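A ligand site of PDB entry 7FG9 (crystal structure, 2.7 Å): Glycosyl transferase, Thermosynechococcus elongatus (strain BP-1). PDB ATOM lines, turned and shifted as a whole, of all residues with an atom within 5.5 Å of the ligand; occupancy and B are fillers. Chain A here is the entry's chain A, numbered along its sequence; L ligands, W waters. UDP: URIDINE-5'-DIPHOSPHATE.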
ATOM      1  N   ALA A  20      28.841  29.349  36.763  1.00  0.00           N
ATOM      2  CA  ALA A  20      27.849  30.293  36.222  1.00  0.00           C
ATOM      3  C   ALA A  20      27.191  29.680  34.992  1.00  0.00           C
ATOM      4  O   ALA A  20      26.408  28.732  35.172  1.00  0.00           O
ATOM      5  CB  ALA A  20      28.523  31.596  35.899  1.00  0.00           C
ATOM      6  N   TYR A  21      27.484  30.199  33.800  1.00  0.00           N
ATOM      7  CA  TYR A  21      26.828  29.661  32.607  1.00  0.00           C
ATOM      8  C   TYR A  21      27.160  28.188  32.391  1.00  0.00           C
ATOM      9  O   TYR A  21      28.305  27.767  32.567  1.00  0.00           O
ATOM     10  CB  TYR A  21      27.190  30.445  31.350  1.00  0.00           C
ATOM     11  CG  TYR A  21      26.679  29.732  30.119  1.00  0.00           C
ATOM     12  CD1 TYR A  21      25.367  29.921  29.676  1.00  0.00           C
ATOM     13  CD2 TYR A  21      27.473  28.812  29.451  1.00  0.00           C
ATOM     14  CE1 TYR A  21      24.881  29.223  28.586  1.00  0.00           C
ATOM     15  CE2 TYR A  21      27.002  28.107  28.379  1.00  0.00           C
ATOM     16  CZ  TYR A  21      25.712  28.315  27.933  1.00  0.00           C
ATOM     17  OH  TYR A  21      25.271  27.608  26.842  1.00  0.00           O
ATOM     18  N   GLY A  22      26.157  27.422  31.949  1.00  0.00           N
ATOM     19  CA  GLY A  22      26.367  26.046  31.526  1.00  0.00           C
ATOM     20  C   GLY A  22      25.184  25.115  31.771  1.00  0.00           C
ATOM     21  O   GLY A  22      24.977  24.647  32.885  1.00  0.00           O
ATOM     22  N   GLY A  23      24.416  24.845  30.729  1.00  0.00           N
ATOM     23  CA  GLY A  23      23.213  24.048  30.905  1.00  0.00           C
ATOM     24  C   GLY A  23      23.487  22.564  30.951  1.00  0.00           C
ATOM     25  O   GLY A  23      23.120  21.909  31.928  1.00  0.00           O
ATOM     26  N   VAL A  24      24.151  22.044  29.906  1.00  0.00           N
ATOM     27  CA  VAL A  24      24.441  20.608  29.832  1.00  0.00           C
ATOM     28  C   VAL A  24      25.190  20.156  31.078  1.00  0.00           C
ATOM     29  O   VAL A  24      24.825  19.150  31.712  1.00  0.00           O
ATOM     30  CB  VAL A  24      25.214  20.282  28.539  1.00  0.00           C
ATOM     31  CG1 VAL A  24      25.701  18.824  28.543  1.00  0.00           C
ATOM     32  CG2 VAL A  24      24.337  20.507  27.339  1.00  0.00           C
ATOM     33  N   LEU A  26      25.334  21.349  34.059  1.00  0.00           N
ATOM     34  CA  LEU A  26      24.534  21.354  35.277  1.00  0.00           C
ATOM     35  C   LEU A  26      23.695  20.082  35.349  1.00  0.00           C
ATOM     36  O   LEU A  26      23.666  19.394  36.379  1.00  0.00           O
ATOM     37  CB  LEU A  26      23.642  22.596  35.328  1.00  0.00           C
ATOM     38  CG  LEU A  26      22.501  22.741  36.360  1.00  0.00           C
ATOM     39  CD1 LEU A  26      22.951  22.738  37.841  1.00  0.00           C
ATOM     40  CD2 LEU A  26      21.689  24.015  36.069  1.00  0.00           C
ATOM     41  N   LEU A 180      17.733  36.056  31.019  1.00  0.00           N
ATOM     42  CA  LEU A 180      18.848  35.248  31.511  1.00  0.00           C
ATOM     43  C   LEU A 180      19.218  34.243  30.446  1.00  0.00           C
ATOM     44  O   LEU A 180      18.373  33.429  30.025  1.00  0.00           O
ATOM     45  CB  LEU A 180      18.497  34.519  32.811  1.00  0.00           C
ATOM     46  CG  LEU A 180      19.606  33.626  33.353  1.00  0.00           C
ATOM     47  CD1 LEU A 180      20.858  34.439  33.668  1.00  0.00           C
ATOM     48  CD2 LEU A 180      19.139  32.838  34.576  1.00  0.00           C
ATOM     49  N   GLY A 181      20.449  34.295  29.992  1.00  0.00           N
ATOM     50  CA  GLY A 181      20.858  33.427  28.897  1.00  0.00           C
ATOM     51  C   GLY A 181      22.068  33.985  28.202  1.00  0.00           C
ATOM     52  O   GLY A 181      22.483  35.127  28.420  1.00  0.00           O
ATOM     53  N   ARG A 182      22.657  33.147  27.368  1.00  0.00           N
ATOM     54  CA  ARG A 182      23.748  33.618  26.531  1.00  0.00           C
ATOM     55  C   ARG A 182      23.239  34.663  25.543  1.00  0.00           C
ATOM     56  O   ARG A 182      22.156  34.547  24.983  1.00  0.00           O
ATOM     57  CB  ARG A 182      24.418  32.442  25.827  1.00  0.00           C
ATOM     58  CG  ARG A 182      23.492  31.651  24.983  1.00  0.00           C
ATOM     59  CD  ARG A 182      24.197  30.432  24.430  1.00  0.00           C
ATOM     60  NE  ARG A 182      23.691  30.169  23.085  1.00  0.00           N
ATOM     61  CZ  ARG A 182      22.821  29.218  22.788  1.00  0.00           C
ATOM     62  NH1 ARG A 182      22.392  28.397  23.724  1.00  0.00           N
ATOM     63  NH2 ARG A 182      22.400  29.085  21.532  1.00  0.00           N
ATOM     64  N   LYS A 187      18.695  33.365  21.348  1.00  0.00           N
ATOM     65  CA  LYS A 187      18.010  33.655  22.595  1.00  0.00           C
ATOM     66  C   LYS A 187      17.233  34.957  22.548  1.00  0.00           C
ATOM     67  O   LYS A 187      16.483  35.234  23.494  1.00  0.00           O
ATOM     68  CB  LYS A 187      19.025  33.717  23.747  1.00  0.00           C
ATOM     69  CG  LYS A 187      19.717  32.387  23.991  1.00  0.00           C
ATOM     70  CD  LYS A 187      18.743  31.241  24.285  1.00  0.00           C
ATOM     71  CE  LYS A 187      19.496  29.898  24.316  1.00  0.00           C
ATOM     72  NZ  LYS A 187      18.858  28.822  25.134  1.00  0.00           N
ATOM     73  N   ALA A 206      21.276  39.478  32.034  1.00  0.00           N
ATOM     74  CA  ALA A 206      22.423  38.732  32.621  1.00  0.00           C
ATOM     75  C   ALA A 206      22.784  37.615  31.642  1.00  0.00           C
ATOM     76  O   ALA A 206      21.869  37.007  31.079  1.00  0.00           O
ATOM     77  CB  ALA A 206      22.111  38.158  33.965  1.00  0.00           C
ATOM     78  N   GLY A 207      24.080  37.345  31.451  1.00  0.00           N
ATOM     79  CA  GLY A 207      24.456  36.251  30.586  1.00  0.00           C
ATOM     80  C   GLY A 207      25.870  36.394  30.048  1.00  0.00           C
ATOM     81  O   GLY A 207      26.639  37.258  30.464  1.00  0.00           O
ATOM     82  N   LYS A 208      26.156  35.551  29.083  1.00  0.00           N
ATOM     83  CA  LYS A 208      27.490  35.255  28.581  1.00  0.00           C
ATOM     84  C   LYS A 208      27.589  35.674  27.118  1.00  0.00           C
ATOM     85  O   LYS A 208      26.626  35.526  26.361  1.00  0.00           O
ATOM     86  CB  LYS A 208      27.730  33.746  28.757  1.00  0.00           C
ATOM     87  CG  LYS A 208      29.024  33.191  28.278  1.00  0.00           C
ATOM     88  CD  LYS A 208      28.835  32.468  26.959  1.00  0.00           C
ATOM     89  CE  LYS A 208      28.186  31.132  27.077  1.00  0.00           C
ATOM     90  NZ  LYS A 208      28.346  30.466  25.729  1.00  0.00           N
ATOM     91  N   GLY A 234      27.006  41.231  33.736  1.00  0.00           N
ATOM     92  CA  GLY A 234      27.098  40.085  32.851  1.00  0.00           C
ATOM     93  C   GLY A 234      27.445  38.800  33.586  1.00  0.00           C
ATOM     94  O   GLY A 234      28.122  38.807  34.618  1.00  0.00           O
ATOM     95  N   GLU A 235      26.981  37.689  33.025  1.00  0.00           N
ATOM     96  CA  GLU A 235      27.234  36.325  33.508  1.00  0.00           C
ATOM     97  C   GLU A 235      27.130  36.155  35.029  1.00  0.00           C
ATOM     98  O   GLU A 235      28.027  36.524  35.787  1.00  0.00           O
ATOM     99  CB  GLU A 235      28.587  35.812  33.039  1.00  0.00           C
ATOM    100  CG  GLU A 235      28.699  34.315  33.333  1.00  0.00           C
ATOM    101  CD  GLU A 235      29.637  33.529  32.417  1.00  0.00           C
ATOM    102  OE1 GLU A 235      30.348  34.131  31.585  1.00  0.00           O
ATOM    103  OE2 GLU A 235      29.671  32.297  32.559  1.00  0.00           O
ATOM    104  N   ALA A 236      26.030  35.526  35.452  1.00  0.00           N
ATOM    105  CA  ALA A 236      25.615  35.462  36.846  1.00  0.00           C
ATOM    106  C   ALA A 236      25.803  34.043  37.385  1.00  0.00           C
ATOM    107  O   ALA A 236      25.573  33.056  36.670  1.00  0.00           O
ATOM    108  CB  ALA A 236      24.145  35.875  36.968  1.00  0.00           C
ATOM    109  N   ASP A 237      26.197  33.946  38.655  1.00  0.00           N
ATOM    110  CA  ASP A 237      26.243  32.641  39.305  1.00  0.00           C
ATOM    111  C   ASP A 237      24.832  32.295  39.833  1.00  0.00           C
ATOM    112  O   ASP A 237      23.839  32.966  39.553  1.00  0.00           O
ATOM    113  CB  ASP A 237      27.313  32.635  40.389  1.00  0.00           C
ATOM    114  CG  ASP A 237      27.045  33.628  41.521  1.00  0.00           C
ATOM    115  OD1 ASP A 237      25.928  34.210  41.614  1.00  0.00           O
ATOM    116  OD2 ASP A 237      27.972  33.814  42.357  1.00  0.00           O
ATOM    117  N   LYS A 241      21.613  34.716  39.753  1.00  0.00           N
ATOM    118  CA  LYS A 241      20.588  34.490  38.747  1.00  0.00           C
ATOM    119  C   LYS A 241      19.260  34.199  39.405  1.00  0.00           C
ATOM    120  O   LYS A 241      18.214  34.623  38.898  1.00  0.00           O
ATOM    121  CB  LYS A 241      20.977  33.357  37.804  1.00  0.00           C
ATOM    122  CG  LYS A 241      20.970  31.964  38.386  1.00  0.00           C
ATOM    123  CD  LYS A 241      21.254  30.945  37.296  1.00  0.00           C
ATOM    124  CE  LYS A 241      21.611  29.584  37.891  1.00  0.00           C
ATOM    125  NZ  LYS A 241      21.430  28.488  36.925  1.00  0.00           N
ATOM    126  N   PHE A 253      11.534  35.295  27.234  1.00  0.00           N
ATOM    127  CA  PHE A 253      12.197  34.174  26.564  1.00  0.00           C
ATOM    128  C   PHE A 253      11.878  34.237  25.077  1.00  0.00           C
ATOM    129  O   PHE A 253      11.240  33.336  24.514  1.00  0.00           O
ATOM    130  CB  PHE A 253      11.786  32.845  27.191  1.00  0.00           C
ATOM    131  CG  PHE A 253      12.680  31.708  26.821  1.00  0.00           C
ATOM    132  CD1 PHE A 253      14.004  31.705  27.216  1.00  0.00           C
ATOM    133  CD2 PHE A 253      12.197  30.646  26.070  1.00  0.00           C
ATOM    134  CE1 PHE A 253      14.852  30.663  26.892  1.00  0.00           C
ATOM    135  CE2 PHE A 253      13.053  29.593  25.729  1.00  0.00           C
ATOM    136  CZ  PHE A 253      14.378  29.612  26.144  1.00  0.00           C
ATOM    137  N   TRP A 257      14.817  30.325  17.760  1.00  0.00           N
ATOM    138  CA  TRP A 257      15.557  29.073  17.534  1.00  0.00           C
ATOM    139  C   TRP A 257      14.688  27.853  17.795  1.00  0.00           C
ATOM    140  O   TRP A 257      13.673  27.990  18.486  1.00  0.00           O
ATOM    141  CB  TRP A 257      16.635  29.137  18.614  1.00  0.00           C
ATOM    142  CG  TRP A 257      17.780  28.179  18.576  1.00  0.00           C
ATOM    143  CD1 TRP A 257      18.429  27.695  17.488  1.00  0.00           C
ATOM    144  CD2 TRP A 257      18.456  27.646  19.723  1.00  0.00           C
ATOM    145  NE1 TRP A 257      19.463  26.887  17.889  1.00  0.00           N
ATOM    146  CE2 TRP A 257      19.499  26.829  19.250  1.00  0.00           C
ATOM    147  CE3 TRP A 257      18.279  27.781  21.100  1.00  0.00           C
ATOM    148  CZ2 TRP A 257      20.355  26.142  20.098  1.00  0.00           C
ATOM    149  CZ3 TRP A 257      19.126  27.093  21.944  1.00  0.00           C
ATOM    150  CH2 TRP A 257      20.145  26.294  21.449  1.00  0.00           C
ATOM    151  N   GLU A 259      14.784  25.792  20.033  1.00  0.00           N
ATOM    152  CA  GLU A 259      15.336  25.530  21.358  1.00  0.00           C
ATOM    153  C   GLU A 259      15.159  24.066  21.763  1.00  0.00           C
ATOM    154  O   GLU A 259      14.019  23.560  21.759  1.00  0.00           O
ATOM    155  CB  GLU A 259      14.669  26.441  22.390  1.00  0.00           C
ATOM    156  CG  GLU A 259      15.046  26.108  23.800  1.00  0.00           C
ATOM    157  CD  GLU A 259      16.403  26.696  24.176  1.00  0.00           C
ATOM    158  OE1 GLU A 259      16.593  27.918  23.946  1.00  0.00           O
ATOM    159  OE2 GLU A 259      17.265  25.941  24.693  1.00  0.00           O
ATOM    160  N   PRO A 260      16.245  23.362  22.109  1.00  0.00           N
ATOM    161  CA  PRO A 260      16.083  21.962  22.547  1.00  0.00           C
ATOM    162  C   PRO A 260      15.304  21.815  23.835  1.00  0.00           C
ATOM    163  O   PRO A 260      14.373  20.997  23.914  1.00  0.00           O
ATOM    164  CB  PRO A 260      17.550  21.501  22.715  1.00  0.00           C
ATOM    165  CG  PRO A 260      18.337  22.383  21.776  1.00  0.00           C
ATOM    166  CD  PRO A 260      17.655  23.715  21.909  1.00  0.00           C
ATOM    167  N   PHE A 261      15.661  22.576  24.861  1.00  0.00           N
ATOM    168  CA  PHE A 261      14.883  22.511  26.086  1.00  0.00           C
ATOM    169  C   PHE A 261      14.672  23.912  26.638  1.00  0.00           C
ATOM    170  O   PHE A 261      13.607  24.491  26.435  1.00  0.00           O
ATOM    171  CB  PHE A 261      15.526  21.604  27.128  1.00  0.00           C
ATOM    172  CG  PHE A 261      14.684  21.437  28.337  1.00  0.00           C
ATOM    173  CD1 PHE A 261      13.646  20.510  28.348  1.00  0.00           C
ATOM    174  CD2 PHE A 261      14.871  22.257  29.446  1.00  0.00           C
ATOM    175  CE1 PHE A 261      12.835  20.372  29.457  1.00  0.00           C
ATOM    176  CE2 PHE A 261      14.073  22.119  30.550  1.00  0.00           C
ATOM    177  CZ  PHE A 261      13.049  21.182  30.557  1.00  0.00           C
ATOM    178  N   GLY A 262      15.656  24.457  27.349  1.00  0.00           N
ATOM    179  CA  GLY A 262      15.567  25.821  27.848  1.00  0.00           C
ATOM    180  C   GLY A 262      15.468  25.881  29.356  1.00  0.00           C
ATOM    181  O   GLY A 262      14.400  26.182  29.897  1.00  0.00           O
ATOM    182  N   LEU A 263      16.604  25.628  30.037  1.00  0.00           N
ATOM    183  CA  LEU A 263      16.604  25.480  31.491  1.00  0.00           C
ATOM    184  C   LEU A 263      16.145  26.747  32.201  1.00  0.00           C
ATOM    185  O   LEU A 263      15.497  26.674  33.254  1.00  0.00           O
ATOM    186  CB  LEU A 263      17.998  25.084  31.971  1.00  0.00           C
ATOM    187  CG  LEU A 263      18.428  23.620  32.006  1.00  0.00           C
ATOM    188  CD1 LEU A 263      19.851  23.497  32.589  1.00  0.00           C
ATOM    189  CD2 LEU A 263      17.430  22.716  32.756  1.00  0.00           C
ATOM    190  N   VAL A 264      16.506  27.904  31.659  1.00  0.00           N
ATOM    191  CA  VAL A 264      16.188  29.206  32.318  1.00  0.00           C
ATOM    192  C   VAL A 264      14.683  29.350  32.552  1.00  0.00           C
ATOM    193  O   VAL A 264      14.312  30.095  33.448  1.00  0.00           O
ATOM    194  CB  VAL A 264      16.769  30.375  31.519  1.00  0.00           C
ATOM    195  CG1 VAL A 264      18.284  30.371  31.547  1.00  0.00           C
ATOM    196  CG2 VAL A 264      16.264  30.383  30.089  1.00  0.00           C
ATOM    197  N   MET A 265      13.855  28.657  31.773  1.00  0.00           N
ATOM    198  CA  MET A 265      12.390  28.771  31.919  1.00  0.00           C
ATOM    199  C   MET A 265      11.967  28.081  33.205  1.00  0.00           C
ATOM    200  O   MET A 265      11.198  28.667  33.955  1.00  0.00           O
ATOM    201  CB  MET A 265      11.676  28.094  30.749  1.00  0.00           C
ATOM    202  CG  MET A 265      12.002  28.657  29.402  1.00  0.00           C
ATOM    203  SD  MET A 265      11.604  27.428  28.147  1.00  0.00           S
ATOM    204  CE  MET A 265      10.019  28.048  27.602  1.00  0.00           C
ATOM    205  N   GLU A 267      13.946  27.424  35.640  1.00  0.00           N
ATOM    206  CA  GLU A 267      14.643  28.133  36.744  1.00  0.00           C
ATOM    207  C   GLU A 267      13.820  29.347  37.169  1.00  0.00           C
ATOM    208  O   GLU A 267      13.768  29.623  38.366  1.00  0.00           O
ATOM    209  CB  GLU A 267      16.060  28.511  36.324  1.00  0.00           C
ATOM    210  CG  GLU A 267      17.024  27.357  36.426  1.00  0.00           C
ATOM    211  CD  GLU A 267      18.241  27.471  35.542  1.00  0.00           C
ATOM    212  OE1 GLU A 267      18.316  28.441  34.774  1.00  0.00           O
ATOM    213  OE2 GLU A 267      19.115  26.598  35.639  1.00  0.00           O
HETATM  214  N1  UDP L   1      23.196  30.638  33.122  1.00  0.00           N
HETATM  215  C2  UDP L   1      23.901  31.238  34.143  1.00  0.00           C
HETATM  216  N3  UDP L   1      24.340  32.416  34.050  1.00  0.00           N
HETATM  217  C4  UDP L   1      24.230  33.182  33.081  1.00  0.00           C
HETATM  218  C5  UDP L   1      23.592  32.854  31.971  1.00  0.00           C
HETATM  219  C6  UDP L   1      23.054  31.516  31.984  1.00  0.00           C
HETATM  220  O2  UDP L   1      24.104  30.618  35.158  1.00  0.00           O
HETATM  221  O4  UDP L   1      24.713  34.289  33.169  1.00  0.00           O
HETATM  222  C1' UDP L   1      22.719  29.327  33.192  1.00  0.00           C
HETATM  223  C2' UDP L   1      21.236  29.232  33.178  1.00  0.00           C
HETATM  224  O2' UDP L   1      20.704  29.395  34.540  1.00  0.00           O
HETATM  225  C3' UDP L   1      21.012  27.889  32.693  1.00  0.00           C
HETATM  226  C4' UDP L   1      22.097  27.598  31.708  1.00  0.00           C
HETATM  227  O4' UDP L   1      23.184  28.604  31.951  1.00  0.00           O
HETATM  228  O3' UDP L   1      21.202  26.990  33.821  1.00  0.00           O
HETATM  229  C5' UDP L   1      21.661  27.770  30.301  1.00  0.00           C
HETATM  230  O5' UDP L   1      20.849  26.701  29.933  1.00  0.00           O
HETATM  231  PA  UDP L   1      19.706  26.992  28.785  1.00  0.00           P
HETATM  232  O1A UDP L   1      18.980  25.785  28.360  1.00  0.00           O
HETATM  233  O2A UDP L   1      18.685  27.916  29.320  1.00  0.00           O
HETATM  234  O3A UDP L   1      20.425  27.715  27.515  1.00  0.00           O
HETATM  235  PB  UDP L   1      21.440  26.900  26.526  1.00  0.00           P
HETATM  236  O1B UDP L   1      20.650  26.482  25.151  1.00  0.00           O
HETATM  237  O2B UDP L   1      22.619  27.743  26.301  1.00  0.00           O
HETATM  238  O3B UDP L   1      21.928  25.690  27.205  1.00  0.00           O
HETATM  239  O   HOH W   1      18.649  30.468  27.591  1.00  0.00           O
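NZ of Lys 187 lies within salt-bridge range of OE1 of Glu 259, at 2.7 Å.
N of Gly 262 lies within hydrogen-bond range of OE2 of Glu 259 (3.4 Å).
The backbone NH (N) of Tyr 21 is in hydrogen-bond range of the side-chain carboxylate (OE2) of Glu 235.
The backbone NH of Gly 181 lies within hydrogen-bond range of the backbone carbonyl oxygen of Ala 206 (3.2 Å).
The side-chain carboxylate (OE2) of Glu 267 lies within salt-bridge range of the side-chain amino group (NZ) of Lys 241.
The backbone carbonyl oxygen of Gly 207 is in hydrogen-bond range of the backbone NH of Glu 235 (2.6 Å).
The backbone carbonyl oxygen (O) of Ala 20 sits close to an oxygen (O2) of the ligand (3.0 Å).
The side-chain carboxylate of Glu 259 lies close to an oxygen (O1B) of the ligand.
Merely in contact with the ligand: Gly 207 (3.3 Å), Glu 235 (3.3 Å), Gly 262 (3.5 Å), Leu 180 (3.6 Å), Trp 257 (3.6 Å), Gly 23 (3.7 Å), Leu 26 (3.8 Å) and Gly 181 (3.98 Å).
Of the 28 residues printed, 19 come within 4 Å of the ligand.
Along chain A the residues within 4 Å of the ligand span positions 20 to 267.
The nearest printed residue that does not touch the ligand is Ala 206 (4.1 Å).
An oxygen (O2') of the ligand lies within hydrogen-bond range of the side-chain carboxylate (OE1) of Glu 267 (2.6 Å).
An oxygen (O4') of the ligand lies within hydrogen-bond range of the backbone NH of Gly 22 (3.2 Å).
NZ of Lys 241 is in hydrogen-bond range of O2' of the ligand, at 2.7 Å.
NZ of Lys 187 is in salt-bridge range of O1B of the ligand, 2.9 Å away.
An oxygen (O1A) of the ligand is in hydrogen-bond range of the backbone NH of Leu 263 (2.9 Å).
O4 of the ligand is in hydrogen-bond range of N of Ala 236 (2.9 Å).
O of Ala 236 is in hydrogen-bond range of N3 of the ligand.
The side-chain hydroxyl (OH) of Tyr 21 sits at hydrogen-bond distance from an oxygen (O2B) of the ligand (2.7 Å).
NH1 of Arg 182 lies within salt-bridge range of O2B of the ligand (2.7 Å).
An oxygen (O2A) of the ligand lies within hydrogen-bond range of the backbone NH of Val 264 (3.2 Å).
Water W1 lies within hydrogen-bond range of NZ of Lys 187 (3.0 Å) and O2A of the ligand (3.1 Å).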
